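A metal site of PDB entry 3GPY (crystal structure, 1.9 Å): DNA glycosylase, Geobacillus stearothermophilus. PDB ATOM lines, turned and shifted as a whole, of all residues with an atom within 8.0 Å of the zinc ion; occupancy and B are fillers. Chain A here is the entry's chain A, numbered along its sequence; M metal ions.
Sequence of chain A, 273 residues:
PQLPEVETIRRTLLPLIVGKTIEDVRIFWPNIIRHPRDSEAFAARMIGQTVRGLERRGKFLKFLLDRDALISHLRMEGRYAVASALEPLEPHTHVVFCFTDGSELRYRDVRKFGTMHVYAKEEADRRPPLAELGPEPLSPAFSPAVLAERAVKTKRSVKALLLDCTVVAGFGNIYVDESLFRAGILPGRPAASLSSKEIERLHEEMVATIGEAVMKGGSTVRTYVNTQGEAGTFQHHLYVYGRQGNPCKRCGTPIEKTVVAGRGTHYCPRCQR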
ATOM      1  N   PHE A 181     -27.330  18.732  20.846  1.00  0.00           N
ATOM      2  CA  PHE A 181     -27.121  18.837  22.287  1.00  0.00           C
ATOM      3  C   PHE A 181     -26.386  17.605  22.819  1.00  0.00           C
ATOM      4  O   PHE A 181     -25.383  17.712  23.558  1.00  0.00           O
ATOM      5  CB  PHE A 181     -28.417  19.022  23.071  1.00  0.00           C
ATOM      6  CG  PHE A 181     -28.235  18.853  24.574  1.00  0.00           C
ATOM      7  CD1 PHE A 181     -27.777  19.911  25.355  1.00  0.00           C
ATOM      8  CD2 PHE A 181     -28.426  17.587  25.175  1.00  0.00           C
ATOM      9  CE1 PHE A 181     -27.592  19.756  26.738  1.00  0.00           C
ATOM     10  CE2 PHE A 181     -28.214  17.421  26.551  1.00  0.00           C
ATOM     11  CZ  PHE A 181     -27.811  18.515  27.339  1.00  0.00           C
ATOM     12  N   TYR A 239     -33.929  17.105  25.828  1.00  0.00           N
ATOM     13  CA  TYR A 239     -33.019  17.915  26.613  1.00  0.00           C
ATOM     14  C   TYR A 239     -33.172  19.413  26.357  1.00  0.00           C
ATOM     15  O   TYR A 239     -32.982  20.234  27.263  1.00  0.00           O
ATOM     16  CB  TYR A 239     -31.590  17.521  26.292  1.00  0.00           C
ATOM     17  CG  TYR A 239     -31.207  16.181  26.839  1.00  0.00           C
ATOM     18  CD1 TYR A 239     -30.868  16.034  28.197  1.00  0.00           C
ATOM     19  CD2 TYR A 239     -31.146  15.051  26.010  1.00  0.00           C
ATOM     20  CE1 TYR A 239     -30.491  14.808  28.698  1.00  0.00           C
ATOM     21  CE2 TYR A 239     -30.778  13.804  26.509  1.00  0.00           C
ATOM     22  CZ  TYR A 239     -30.445  13.709  27.854  1.00  0.00           C
ATOM     23  OH  TYR A 239     -30.074  12.489  28.367  1.00  0.00           O
ATOM     24  N   VAL A 240     -33.476  19.758  25.111  1.00  0.00           N
ATOM     25  CA  VAL A 240     -33.464  21.170  24.703  1.00  0.00           C
ATOM     26  C   VAL A 240     -34.711  21.657  23.966  1.00  0.00           C
ATOM     27  O   VAL A 240     -35.190  22.767  24.217  1.00  0.00           O
ATOM     28  CB  VAL A 240     -32.145  21.551  23.901  1.00  0.00           C
ATOM     29  CG1 VAL A 240     -30.888  21.399  24.797  1.00  0.00           C
ATOM     30  CG2 VAL A 240     -31.996  20.763  22.569  1.00  0.00           C
ATOM     31  N   PRO A 247     -33.888  25.014  33.096  1.00  0.00           N
ATOM     32  CA  PRO A 247     -32.524  24.554  33.327  1.00  0.00           C
ATOM     33  C   PRO A 247     -32.186  23.361  32.458  1.00  0.00           C
ATOM     34  O   PRO A 247     -33.024  22.471  32.247  1.00  0.00           O
ATOM     35  CB  PRO A 247     -32.543  24.095  34.797  1.00  0.00           C
ATOM     36  CG  PRO A 247     -33.736  24.781  35.411  1.00  0.00           C
ATOM     37  CD  PRO A 247     -34.727  24.856  34.302  1.00  0.00           C
ATOM     38  N   CYS A 248     -30.951  23.338  31.968  1.00  0.00           N
ATOM     39  CA  CYS A 248     -30.417  22.143  31.336  1.00  0.00           C
ATOM     40  C   CYS A 248     -30.478  20.965  32.320  1.00  0.00           C
ATOM     41  O   CYS A 248     -30.136  21.112  33.516  1.00  0.00           O
ATOM     42  CB  CYS A 248     -28.964  22.404  30.907  1.00  0.00           C
ATOM     43  SG  CYS A 248     -28.164  20.976  30.127  1.00  0.00           S
ATOM     44  N   LYS A 249     -30.924  19.810  31.823  1.00  0.00           N
ATOM     45  CA  LYS A 249     -31.059  18.603  32.655  1.00  0.00           C
ATOM     46  C   LYS A 249     -29.690  18.075  33.090  1.00  0.00           C
ATOM     47  O   LYS A 249     -29.583  17.334  34.065  1.00  0.00           O
ATOM     48  CB  LYS A 249     -31.817  17.505  31.879  1.00  0.00           C
ATOM     49  CG  LYS A 249     -33.249  17.869  31.517  1.00  0.00           C
ATOM     50  CD  LYS A 249     -33.985  16.647  30.940  1.00  0.00           C
ATOM     51  CE  LYS A 249     -35.435  16.966  30.628  1.00  0.00           C
ATOM     52  NZ  LYS A 249     -36.053  15.763  30.011  1.00  0.00           N
ATOM     53  N   ARG A 250     -28.648  18.458  32.361  1.00  0.00           N
ATOM     54  CA  ARG A 250     -27.301  18.000  32.635  1.00  0.00           C
ATOM     55  C   ARG A 250     -26.495  18.956  33.509  1.00  0.00           C
ATOM     56  O   ARG A 250     -25.790  18.524  34.423  1.00  0.00           O
ATOM     57  CB  ARG A 250     -26.564  17.746  31.309  1.00  0.00           C
ATOM     58  CG  ARG A 250     -25.124  17.256  31.471  1.00  0.00           C
ATOM     59  N   CYS A 251     -26.580  20.264  33.239  1.00  0.00           N
ATOM     60  CA  CYS A 251     -25.722  21.217  33.949  1.00  0.00           C
ATOM     61  C   CYS A 251     -26.483  22.355  34.675  1.00  0.00           C
ATOM     62  O   CYS A 251     -25.872  23.144  35.402  1.00  0.00           O
ATOM     63  CB  CYS A 251     -24.688  21.817  32.988  1.00  0.00           C
ATOM     64  SG  CYS A 251     -25.393  23.025  31.823  1.00  0.00           S
ATOM     65  N   GLY A 252     -27.797  22.426  34.473  1.00  0.00           N
ATOM     66  CA  GLY A 252     -28.616  23.459  35.104  1.00  0.00           C
ATOM     67  C   GLY A 252     -28.589  24.842  34.457  1.00  0.00           C
ATOM     68  O   GLY A 252     -29.336  25.728  34.895  1.00  0.00           O
ATOM     69  N   THR A 253     -27.757  25.045  33.432  1.00  0.00           N
ATOM     70  CA  THR A 253     -27.698  26.343  32.724  1.00  0.00           C
ATOM     71  C   THR A 253     -29.017  26.523  31.965  1.00  0.00           C
ATOM     72  O   THR A 253     -29.500  25.550  31.380  1.00  0.00           O
ATOM     73  CB  THR A 253     -26.525  26.368  31.699  1.00  0.00           C
ATOM     74  OG1 THR A 253     -25.308  26.112  32.404  1.00  0.00           O
ATOM     75  CG2 THR A 253     -26.409  27.733  30.956  1.00  0.00           C
ATOM     76  N   PRO A 254     -29.603  27.755  31.969  1.00  0.00           N
ATOM     77  CA  PRO A 254     -30.866  27.908  31.209  1.00  0.00           C
ATOM     78  C   PRO A 254     -30.681  27.641  29.724  1.00  0.00           C
ATOM     79  O   PRO A 254     -29.716  28.122  29.106  1.00  0.00           O
ATOM     80  CB  PRO A 254     -31.241  29.401  31.414  1.00  0.00           C
ATOM     81  CG  PRO A 254     -30.549  29.779  32.729  1.00  0.00           C
ATOM     82  CD  PRO A 254     -29.243  29.004  32.680  1.00  0.00           C
ATOM     83  N   ILE A 255     -31.602  26.868  29.158  1.00  0.00           N
ATOM     84  CA  ILE A 255     -31.625  26.567  27.737  1.00  0.00           C
ATOM     85  C   ILE A 255     -31.962  27.857  26.987  1.00  0.00           C
ATOM     86  O   ILE A 255     -32.823  28.631  27.403  1.00  0.00           O
ATOM     87  CB  ILE A 255     -32.616  25.416  27.408  1.00  0.00           C
ATOM     88  CG1 ILE A 255     -32.212  24.140  28.183  1.00  0.00           C
ATOM     89  CG2 ILE A 255     -32.739  25.196  25.886  1.00  0.00           C
ATOM     90  CD1 ILE A 255     -30.701  23.727  27.973  1.00  0.00           C
ATOM     91  N   TYR A 267     -30.647  25.235  22.550  1.00  0.00           N
ATOM     92  CA  TYR A 267     -29.318  24.723  22.870  1.00  0.00           C
ATOM     93  C   TYR A 267     -28.933  25.101  24.315  1.00  0.00           C
ATOM     94  O   TYR A 267     -29.462  26.067  24.887  1.00  0.00           O
ATOM     95  CB  TYR A 267     -28.261  25.209  21.842  1.00  0.00           C
ATOM     96  CG  TYR A 267     -28.126  26.711  21.881  1.00  0.00           C
ATOM     97  CD1 TYR A 267     -27.146  27.310  22.672  1.00  0.00           C
ATOM     98  CD2 TYR A 267     -29.026  27.541  21.177  1.00  0.00           C
ATOM     99  CE1 TYR A 267     -27.046  28.686  22.770  1.00  0.00           C
ATOM    100  CE2 TYR A 267     -28.919  28.944  21.264  1.00  0.00           C
ATOM    101  CZ  TYR A 267     -27.934  29.497  22.055  1.00  0.00           C
ATOM    102  OH  TYR A 267     -27.811  30.863  22.170  1.00  0.00           O
ATOM    103  N   CYS A 268     -28.031  24.316  24.883  1.00  0.00           N
ATOM    104  CA  CYS A 268     -27.353  24.681  26.137  1.00  0.00           C
ATOM    105  C   CYS A 268     -26.014  25.302  25.820  1.00  0.00           C
ATOM    106  O   CYS A 268     -25.129  24.617  25.264  1.00  0.00           O
ATOM    107  CB  CYS A 268     -27.135  23.445  27.028  1.00  0.00           C
ATOM    108  SG  CYS A 268     -26.248  23.888  28.534  1.00  0.00           S
ATOM    109  N   PRO A 269     -25.802  26.579  26.208  1.00  0.00           N
ATOM    110  CA  PRO A 269     -24.565  27.238  25.856  1.00  0.00           C
ATOM    111  C   PRO A 269     -23.358  26.694  26.646  1.00  0.00           C
ATOM    112  O   PRO A 269     -22.236  27.062  26.340  1.00  0.00           O
ATOM    113  CB  PRO A 269     -24.825  28.710  26.215  1.00  0.00           C
ATOM    114  CG  PRO A 269     -25.789  28.653  27.333  1.00  0.00           C
ATOM    115  CD  PRO A 269     -26.680  27.445  27.029  1.00  0.00           C
ATOM    116  N   ARG A 270     -23.587  25.848  27.653  1.00  0.00           N
ATOM    117  CA  ARG A 270     -22.482  25.244  28.382  1.00  0.00           C
ATOM    118  C   ARG A 270     -22.123  23.843  27.859  1.00  0.00           C
ATOM    119  O   ARG A 270     -20.950  23.537  27.637  1.00  0.00           O
ATOM    120  CB  ARG A 270     -22.738  25.236  29.916  1.00  0.00           C
ATOM    121  CG  ARG A 270     -21.644  24.519  30.717  1.00  0.00           C
ATOM    122  CD  ARG A 270     -21.963  24.497  32.202  1.00  0.00           C
ATOM    123  NE  ARG A 270     -20.828  23.999  32.959  1.00  0.00           N
ATOM    124  CZ  ARG A 270     -20.668  24.115  34.274  1.00  0.00           C
ATOM    125  NH1 ARG A 270     -19.562  23.633  34.827  1.00  0.00           N
ATOM    126  NH2 ARG A 270     -21.571  24.742  35.017  1.00  0.00           N
ATOM    127  N   CYS A 271     -23.137  23.004  27.649  1.00  0.00           N
ATOM    128  CA  CYS A 271     -22.916  21.641  27.213  1.00  0.00           C
ATOM    129  C   CYS A 271     -22.501  21.596  25.733  1.00  0.00           C
ATOM    130  O   CYS A 271     -21.811  20.664  25.307  1.00  0.00           O
ATOM    131  CB  CYS A 271     -24.172  20.781  27.410  1.00  0.00           C
ATOM    132  SG  CYS A 271     -24.522  20.402  29.146  1.00  0.00           S
ATOM    133  N   GLN A 272     -22.941  22.569  24.943  1.00  0.00           N
ATOM    134  CA  GLN A 272     -22.616  22.608  23.513  1.00  0.00           C
ATOM    135  C   GLN A 272     -21.536  23.629  23.206  1.00  0.00           C
ATOM    136  O   GLN A 272     -21.589  24.757  23.700  1.00  0.00           O
ATOM    137  CB  GLN A 272     -23.861  22.876  22.674  1.00  0.00           C
ATOM    138  CG  GLN A 272     -24.856  21.713  22.775  1.00  0.00           C
ATOM    139  CD  GLN A 272     -26.233  22.068  22.262  1.00  0.00           C
ATOM    140  OE1 GLN A 272     -27.135  22.314  23.050  1.00  0.00           O
ATOM    141  NE2 GLN A 272     -26.418  22.068  20.943  1.00  0.00           N
HETATM  142 ZN    ZN M   1     -26.065  22.008  29.826  1.00  0.00          ZN
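SG of Cys 268 sits close to N of Arg 270.
The backbone NH of Cys 268 sits at hydrogen-bond distance from the side-chain amide oxygen of Gln 272.
The side-chain sulfur (SG) of Cys 251 sits close to the side-chain hydroxyl (OG1) of Thr 253 (3.1 Å).
N of Arg 250 sits close to SG of Cys 248, 3.4 Å away.
The backbone NH of Cys 248 sits at hydrogen-bond distance from the backbone carbonyl oxygen of Thr 253.
Of the 18 residues printed, 4 come within 4 Å of the zinc ion.
The nearest printed residue that does not touch the zinc ion is Phe 181 (4.1 Å).
SG of Cys 268 binds the zinc ion (2.3 Å).
SG of Cys 271 is bound to the zinc ion (2.3 Å).
The zinc ion is bound by SG of Cys 251, at 2.3 Å.
SG of Cys 248 binds the zinc ion (2.4 Å).
The zinc ion has four donor atoms within binding distance.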
